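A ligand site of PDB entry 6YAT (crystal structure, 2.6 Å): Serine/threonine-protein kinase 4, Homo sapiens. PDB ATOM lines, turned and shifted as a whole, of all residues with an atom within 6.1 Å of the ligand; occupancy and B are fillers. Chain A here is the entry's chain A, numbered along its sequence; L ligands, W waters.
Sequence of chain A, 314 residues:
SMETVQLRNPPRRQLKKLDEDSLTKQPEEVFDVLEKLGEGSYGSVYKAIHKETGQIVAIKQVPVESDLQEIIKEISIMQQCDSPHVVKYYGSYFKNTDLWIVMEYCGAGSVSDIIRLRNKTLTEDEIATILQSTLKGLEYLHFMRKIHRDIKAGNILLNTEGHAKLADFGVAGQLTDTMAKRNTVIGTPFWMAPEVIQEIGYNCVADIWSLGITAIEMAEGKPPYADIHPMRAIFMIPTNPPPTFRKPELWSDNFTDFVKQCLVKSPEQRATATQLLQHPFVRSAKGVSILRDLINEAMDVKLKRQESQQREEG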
ATOM      1  N   LEU A  37      21.854   1.947 -30.516  1.00  0.00           N
ATOM      2  CA  LEU A  37      21.712   2.282 -29.077  1.00  0.00           C
ATOM      3  C   LEU A  37      20.303   1.958 -28.619  1.00  0.00           C
ATOM      4  O   LEU A  37      20.137   1.560 -27.420  1.00  0.00           O
ATOM      5  CB  LEU A  37      22.041   3.760 -28.870  1.00  0.00           C
ATOM      6  CG  LEU A  37      23.471   4.174 -29.212  1.00  0.00           C
ATOM      7  CD1 LEU A  37      23.659   5.679 -29.096  1.00  0.00           C
ATOM      8  CD2 LEU A  37      24.481   3.447 -28.354  1.00  0.00           C
ATOM      9  N   GLY A  38      19.316   2.111 -29.519  1.00  0.00           N
ATOM     10  CA  GLY A  38      17.901   1.727 -29.274  1.00  0.00           C
ATOM     11  C   GLY A  38      16.955   2.334 -30.307  1.00  0.00           C
ATOM     12  O   GLY A  38      17.458   2.810 -31.346  1.00  0.00           O
ATOM     13  N   GLU A  39      15.649   2.259 -30.044  1.00  0.00           N
ATOM     14  CA  GLU A  39      14.571   2.806 -30.896  1.00  0.00           C
ATOM     15  C   GLU A  39      14.233   4.219 -30.432  1.00  0.00           C
ATOM     16  O   GLU A  39      14.367   4.510 -29.226  1.00  0.00           O
ATOM     17  CB  GLU A  39      13.311   1.934 -30.826  1.00  0.00           C
ATOM     18  CG  GLU A  39      13.528   0.511 -31.309  1.00  0.00           C
ATOM     19  CD  GLU A  39      13.891   0.385 -32.780  1.00  0.00           C
ATOM     20  OE1 GLU A  39      13.445   1.239 -33.572  1.00  0.00           O
ATOM     21  OE2 GLU A  39      14.628  -0.547 -33.120  1.00  0.00           O
ATOM     22  N   GLY A  40      13.883   5.091 -31.382  1.00  0.00           N
ATOM     23  CA  GLY A  40      13.315   6.411 -31.118  1.00  0.00           C
ATOM     24  C   GLY A  40      11.952   6.526 -31.717  1.00  0.00           C
ATOM     25  O   GLY A  40      11.499   5.546 -32.342  1.00  0.00           O
ATOM     26  N   SER A  41      11.373   7.725 -31.663  1.00  0.00           N
ATOM     27  CA  SER A  41       9.992   8.023 -32.110  1.00  0.00           C
ATOM     28  C   SER A  41       9.654   7.276 -33.413  1.00  0.00           C
ATOM     29  O   SER A  41       8.788   6.366 -33.355  1.00  0.00           O
ATOM     30  CB  SER A  41       9.798   9.501 -32.253  1.00  0.00           C
ATOM     31  OG  SER A  41      10.177  10.173 -31.068  1.00  0.00           O
ATOM     32  N   VAL A  45      18.273   4.543 -33.402  1.00  0.00           N
ATOM     33  CA  VAL A  45      19.310   5.524 -32.968  1.00  0.00           C
ATOM     34  C   VAL A  45      20.658   4.804 -32.834  1.00  0.00           C
ATOM     35  O   VAL A  45      20.685   3.737 -32.197  1.00  0.00           O
ATOM     36  CB  VAL A  45      18.913   6.220 -31.650  1.00  0.00           C
ATOM     37  CG1 VAL A  45      19.938   7.251 -31.224  1.00  0.00           C
ATOM     38  CG2 VAL A  45      17.546   6.856 -31.750  1.00  0.00           C
ATOM     39  N   ALA A  58      24.874  10.869 -31.260  1.00  0.00           N
ATOM     40  CA  ALA A  58      23.794   9.909 -31.571  1.00  0.00           C
ATOM     41  C   ALA A  58      23.048  10.389 -32.813  1.00  0.00           C
ATOM     42  O   ALA A  58      22.866  11.598 -32.961  1.00  0.00           O
ATOM     43  CB  ALA A  58      22.857   9.786 -30.377  1.00  0.00           C
ATOM     44  N   LYS A  60      19.507   9.422 -34.984  1.00  0.00           N
ATOM     45  CA  LYS A  60      18.234   8.743 -35.332  1.00  0.00           C
ATOM     46  C   LYS A  60      18.079   8.729 -36.844  1.00  0.00           C
ATOM     47  O   LYS A  60      18.176   9.786 -37.451  1.00  0.00           O
ATOM     48  CB  LYS A  60      17.060   9.469 -34.668  1.00  0.00           C
ATOM     49  CG  LYS A  60      15.696   8.847 -34.932  1.00  0.00           C
ATOM     50  CD  LYS A  60      14.696   9.127 -33.833  1.00  0.00           C
ATOM     51  CE  LYS A  60      13.425   9.791 -34.322  1.00  0.00           C
ATOM     52  NZ  LYS A  60      12.892  10.724 -33.301  1.00  0.00           N
ATOM     53  N   GLU A  74       9.523  17.521 -33.751  1.00  0.00           N
ATOM     54  CA  GLU A  74      10.524  17.016 -32.776  1.00  0.00           C
ATOM     55  C   GLU A  74      11.788  17.862 -32.872  1.00  0.00           C
ATOM     56  O   GLU A  74      12.288  18.331 -31.791  1.00  0.00           O
ATOM     57  CB  GLU A  74      10.835  15.541 -33.025  1.00  0.00           C
ATOM     58  CG  GLU A  74      12.123  15.083 -32.370  1.00  0.00           C
ATOM     59  CD  GLU A  74      12.318  13.573 -32.312  1.00  0.00           C
ATOM     60  OE1 GLU A  74      11.827  12.873 -33.232  1.00  0.00           O
ATOM     61  OE2 GLU A  74      12.965  13.098 -31.329  1.00  0.00           O
ATOM     62  N   MET A  78      13.385  20.518 -30.124  1.00  0.00           N
ATOM     63  CA  MET A  78      14.785  20.300 -29.657  1.00  0.00           C
ATOM     64  C   MET A  78      15.612  21.578 -29.885  1.00  0.00           C
ATOM     65  O   MET A  78      16.405  21.912 -29.027  1.00  0.00           O
ATOM     66  CB  MET A  78      15.433  19.127 -30.373  1.00  0.00           C
ATOM     67  CG  MET A  78      15.008  17.789 -29.819  1.00  0.00           C
ATOM     68  SD  MET A  78      16.243  16.515 -30.091  1.00  0.00           S
ATOM     69  CE  MET A  78      15.669  15.864 -31.653  1.00  0.00           C
ATOM     70  N   VAL A  87      18.503  16.943 -24.196  1.00  0.00           N
ATOM     71  CA  VAL A  87      19.457  16.528 -25.277  1.00  0.00           C
ATOM     72  C   VAL A  87      19.441  17.606 -26.349  1.00  0.00           C
ATOM     73  O   VAL A  87      18.337  18.021 -26.740  1.00  0.00           O
ATOM     74  CB  VAL A  87      19.118  15.144 -25.886  1.00  0.00           C
ATOM     75  CG1 VAL A  87      18.999  14.067 -24.816  1.00  0.00           C
ATOM     76  CG2 VAL A  87      17.861  15.173 -26.742  1.00  0.00           C
ATOM     77  N   MET A 103      22.338  14.257 -32.660  1.00  0.00           N
ATOM     78  CA  MET A 103      21.993  14.687 -31.277  1.00  0.00           C
ATOM     79  C   MET A 103      23.184  14.498 -30.336  1.00  0.00           C
ATOM     80  O   MET A 103      24.096  13.704 -30.668  1.00  0.00           O
ATOM     81  CB  MET A 103      20.802  13.896 -30.745  1.00  0.00           C
ATOM     82  CG  MET A 103      19.481  14.386 -31.259  1.00  0.00           C
ATOM     83  SD  MET A 103      18.168  13.172 -31.086  1.00  0.00           S
ATOM     84  CE  MET A 103      18.780  11.847 -32.121  1.00  0.00           C
ATOM     85  N   GLU A 104      23.116  15.158 -29.178  1.00  0.00           N
ATOM     86  CA  GLU A 104      23.954  14.906 -27.983  1.00  0.00           C
ATOM     87  C   GLU A 104      23.943  13.404 -27.654  1.00  0.00           C
ATOM     88  O   GLU A 104      22.829  12.814 -27.601  1.00  0.00           O
ATOM     89  CB  GLU A 104      23.435  15.722 -26.808  1.00  0.00           C
ATOM     90  CG  GLU A 104      24.341  15.718 -25.606  1.00  0.00           C
ATOM     91  CD  GLU A 104      23.813  16.514 -24.430  1.00  0.00           C
ATOM     92  OE1 GLU A 104      22.851  17.277 -24.624  1.00  0.00           O
ATOM     93  OE2 GLU A 104      24.317  16.302 -23.311  1.00  0.00           O
ATOM     94  N   TYR A 105      25.135  12.818 -27.486  1.00  0.00           N
ATOM     95  CA  TYR A 105      25.359  11.429 -27.025  1.00  0.00           C
ATOM     96  C   TYR A 105      25.541  11.427 -25.509  1.00  0.00           C
ATOM     97  O   TYR A 105      26.414  12.163 -25.014  1.00  0.00           O
ATOM     98  CB  TYR A 105      26.596  10.827 -27.701  1.00  0.00           C
ATOM     99  CG  TYR A 105      26.995   9.455 -27.194  1.00  0.00           C
ATOM    100  CD1 TYR A 105      26.204   8.343 -27.455  1.00  0.00           C
ATOM    101  CD2 TYR A 105      28.163   9.267 -26.467  1.00  0.00           C
ATOM    102  CE1 TYR A 105      26.569   7.073 -27.007  1.00  0.00           C
ATOM    103  CE2 TYR A 105      28.532   8.010 -26.025  1.00  0.00           C
ATOM    104  CZ  TYR A 105      27.741   6.907 -26.303  1.00  0.00           C
ATOM    105  OH  TYR A 105      28.097   5.666 -25.852  1.00  0.00           O
ATOM    106  N   CYS A 106      24.750  10.622 -24.806  1.00  0.00           N
ATOM    107  CA  CYS A 106      24.841  10.409 -23.323  1.00  0.00           C
ATOM    108  C   CYS A 106      25.328   8.973 -23.051  1.00  0.00           C
ATOM    109  O   CYS A 106      24.533   8.026 -23.259  1.00  0.00           O
ATOM    110  CB  CYS A 106      23.517  10.717 -22.645  1.00  0.00           C
ATOM    111  SG  CYS A 106      22.829  12.326 -23.124  1.00  0.00           S
ATOM    112  N   GLY A 107      26.581   8.851 -22.582  1.00  0.00           N
ATOM    113  CA  GLY A 107      27.415   7.626 -22.690  1.00  0.00           C
ATOM    114  C   GLY A 107      26.994   6.500 -21.730  1.00  0.00           C
ATOM    115  O   GLY A 107      27.566   5.381 -21.878  1.00  0.00           O
ATOM    116  N   GLY A 109      23.624   5.750 -21.343  1.00  0.00           N
ATOM    117  CA  GLY A 109      22.351   5.292 -21.937  1.00  0.00           C
ATOM    118  C   GLY A 109      21.168   5.707 -21.086  1.00  0.00           C
ATOM    119  O   GLY A 109      21.309   6.649 -20.273  1.00  0.00           O
ATOM    120  N   SER A 110      20.014   5.095 -21.329  1.00  0.00           N
ATOM    121  CA  SER A 110      18.756   5.350 -20.598  1.00  0.00           C
ATOM    122  C   SER A 110      18.805   4.645 -19.217  1.00  0.00           C
ATOM    123  O   SER A 110      19.543   3.654 -19.068  1.00  0.00           O
ATOM    124  CB  SER A 110      17.585   4.897 -21.402  1.00  0.00           C
ATOM    125  OG  SER A 110      17.614   3.480 -21.580  1.00  0.00           O
ATOM    126  N   ASP A 113      17.834   1.051 -19.599  1.00  0.00           N
ATOM    127  CA  ASP A 113      18.985   0.212 -20.028  1.00  0.00           C
ATOM    128  C   ASP A 113      19.849  -0.140 -18.817  1.00  0.00           C
ATOM    129  O   ASP A 113      20.422  -1.256 -18.805  1.00  0.00           O
ATOM    130  CB  ASP A 113      19.825   0.929 -21.092  1.00  0.00           C
ATOM    131  CG  ASP A 113      19.154   0.913 -22.458  1.00  0.00           C
ATOM    132  OD1 ASP A 113      18.333  -0.048 -22.708  1.00  0.00           O
ATOM    133  OD2 ASP A 113      19.424   1.908 -23.274  1.00  0.00           O
ATOM    134  N   GLY A 154      12.896   4.912 -19.916  1.00  0.00           N
ATOM    135  CA  GLY A 154      13.351   4.780 -21.309  1.00  0.00           C
ATOM    136  C   GLY A 154      13.839   6.099 -21.895  1.00  0.00           C
ATOM    137  O   GLY A 154      14.783   6.050 -22.704  1.00  0.00           O
ATOM    138  N   ASN A 155      13.254   7.224 -21.462  1.00  0.00           N
ATOM    139  CA  ASN A 155      13.435   8.556 -22.103  1.00  0.00           C
ATOM    140  C   ASN A 155      14.177   9.512 -21.169  1.00  0.00           C
ATOM    141  O   ASN A 155      14.208  10.707 -21.444  1.00  0.00           O
ATOM    142  CB  ASN A 155      12.095   9.124 -22.554  1.00  0.00           C
ATOM    143  CG  ASN A 155      11.491   8.333 -23.704  1.00  0.00           C
ATOM    144  OD1 ASN A 155      12.233   7.719 -24.476  1.00  0.00           O
ATOM    145  ND2 ASN A 155      10.172   8.263 -23.767  1.00  0.00           N
ATOM    146  N   LEU A 157      18.150   9.941 -19.916  1.00  0.00           N
ATOM    147  CA  LEU A 157      19.508   9.516 -20.294  1.00  0.00           C
ATOM    148  C   LEU A 157      20.501  10.034 -19.256  1.00  0.00           C
ATOM    149  O   LEU A 157      20.245  11.108 -18.697  1.00  0.00           O
ATOM    150  CB  LEU A 157      19.843  10.065 -21.693  1.00  0.00           C
ATOM    151  CG  LEU A 157      18.879   9.679 -22.819  1.00  0.00           C
ATOM    152  CD1 LEU A 157      19.374  10.187 -24.169  1.00  0.00           C
ATOM    153  CD2 LEU A 157      18.686   8.178 -22.865  1.00  0.00           C
ATOM    154  N   ALA A 167      15.079  12.925 -23.211  1.00  0.00           N
ATOM    155  CA  ALA A 167      15.229  12.522 -24.628  1.00  0.00           C
ATOM    156  C   ALA A 167      13.871  12.166 -25.203  1.00  0.00           C
ATOM    157  O   ALA A 167      12.909  11.973 -24.397  1.00  0.00           O
ATOM    158  CB  ALA A 167      16.193  11.366 -24.742  1.00  0.00           C
ATOM    159  N   ASP A 168      13.767  12.152 -26.534  1.00  0.00           N
ATOM    160  CA  ASP A 168      12.627  11.602 -27.309  1.00  0.00           C
ATOM    161  C   ASP A 168      11.466  12.628 -27.313  1.00  0.00           C
ATOM    162  O   ASP A 168      10.469  12.380 -26.604  1.00  0.00           O
ATOM    163  CB  ASP A 168      12.201  10.240 -26.756  1.00  0.00           C
ATOM    164  CG  ASP A 168      11.479   9.377 -27.788  1.00  0.00           C
ATOM    165  OD1 ASP A 168      11.129   9.952 -28.894  1.00  0.00           O
ATOM    166  OD2 ASP A 168      11.269   8.149 -27.500  1.00  0.00           O
ATOM    167  N   PHE A 169      11.549  13.642 -28.157  1.00  0.00           N
ATOM    168  CA  PHE A 169      10.481  14.673 -28.314  1.00  0.00           C
ATOM    169  C   PHE A 169       9.572  14.315 -29.503  1.00  0.00           C
ATOM    170  O   PHE A 169       8.833  15.165 -29.930  1.00  0.00           O
ATOM    171  CB  PHE A 169      11.113  16.054 -28.412  1.00  0.00           C
ATOM    172  CG  PHE A 169      11.735  16.492 -27.119  1.00  0.00           C
ATOM    173  CD1 PHE A 169      13.010  16.078 -26.769  1.00  0.00           C
ATOM    174  CD2 PHE A 169      10.968  17.131 -26.155  1.00  0.00           C
ATOM    175  CE1 PHE A 169      13.547  16.401 -25.527  1.00  0.00           C
ATOM    176  CE2 PHE A 169      11.510  17.476 -24.935  1.00  0.00           C
ATOM    177  CZ  PHE A 169      12.804  17.126 -24.630  1.00  0.00           C
HETATM  178  N1  LIG L   1      22.677   8.784 -26.287  1.00  0.00           N
HETATM  179  C1  LIG L   1      15.791   8.415 -27.136  1.00  0.00           C
HETATM  180  N2  LIG L   1      19.337   6.305 -26.559  1.00  0.00           N
HETATM  181  C2  LIG L   1      17.955   9.211 -27.827  1.00  0.00           C
HETATM  182  C3  LIG L   1      19.406   9.408 -27.571  1.00  0.00           C
HETATM  183  C4  LIG L   1      20.070  10.582 -27.766  1.00  0.00           C
HETATM  184 CL1  LIG L   1      15.246  10.582 -30.437  1.00  0.00          CL
HETATM  185  C5  LIG L   1      16.002   9.713 -29.116  1.00  0.00           C
HETATM  186  C6  LIG L   1      17.364   9.801 -28.941  1.00  0.00           C
HETATM  187  C7  LIG L   1      17.157   8.521 -26.929  1.00  0.00           C
HETATM  188  C8  LIG L   1      15.205   9.008 -28.237  1.00  0.00           C
HETATM  189  C9  LIG L   1      20.378   8.502 -26.977  1.00  0.00           C
HETATM  190  C10 LIG L   1      21.548   9.237 -26.816  1.00  0.00           C
HETATM  191  N3  LIG L   1      21.364  10.490 -27.326  1.00  0.00           N
HETATM  192  C11 LIG L   1      20.447   7.152 -26.544  1.00  0.00           C
HETATM  193  N4  LIG L   1      21.585   6.631 -26.038  1.00  0.00           N
HETATM  194  C12 LIG L   1      22.623   7.498 -25.935  1.00  0.00           C
HETATM  195  C13 LIG L   1      18.689   6.001 -27.838  1.00  0.00           C
HETATM  196  C14 LIG L   1      17.370   5.334 -27.593  1.00  0.00           C
HETATM  197  O1  LIG L   1      17.524   4.144 -26.837  1.00  0.00           O
HETATM  198  C15 LIG L   1      18.110   4.451 -25.591  1.00  0.00           C
HETATM  199  C16 LIG L   1      19.454   5.083 -25.752  1.00  0.00           C
HETATM  200  O   HOH W   1      23.244   4.411 -24.969  1.00  0.00           O
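N of Cys 106 lies within hydrogen-bond range of N1 of the ligand (3.1 Å). O of Glu 104 is in hydrogen-bond range of N3 of the ligand, 2.8 Å away.
Leu 37 touches the ligand (O to O1, 3.7 Å). CA of Gly 38 touches O1 of the ligand, at 3.5 Å. Glu 39 touches the ligand. CG1 of Val 45 touches C13 of the ligand, 3.8 Å away. Ala 58 touches the ligand (CB to N3, 3.5 Å). Lys 60 touches the ligand. OE2 of Glu 74 touches CL1 of the ligand (3.5 Å). SD of Met 103 touches CL1 of the ligand, at 3.96 Å. Tyr 105 touches the ligand (CD1 to N1, 3.7 Å). Asp 113 touches the ligand (OD2 to C15, 3.7 Å). CD1 of Leu 157 touches C9 of the ligand, at 3.4 Å. Ala 167 touches the ligand (CB to C7, 3.7 Å). Asp 168 touches the ligand. Of the 25 residues printed, 15 come within 4 Å of the ligand.
The backbone NH (N) of Leu 37 lies within hydrogen-bond range of the backbone carbonyl oxygen (O) of Val 45 (2.7 Å). The side-chain amide oxygen of Asn 155 sits close to the side-chain carboxylate of Asp 168, 3.2 Å away. O of Asn 155 sits at hydrogen-bond distance from N of Ala 167 (3.0 Å). O of Ala 58 sits at hydrogen-bond distance from N of Met 103, 2.7 Å away. The backbone carbonyl oxygen (O) of Gly 38 sits at hydrogen-bond distance from the backbone NH (N) of Val 45 (2.8 Å). The side-chain hydroxyl (OG) of Ser 110 sits at hydrogen-bond distance from the side-chain carboxylate (OD2) of Asp 113 (2.9 Å). The side-chain carboxylate (OE2) of Glu 74 is in salt-bridge range of the side-chain amino group (NZ) of Lys 60, at 3.1 Å.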
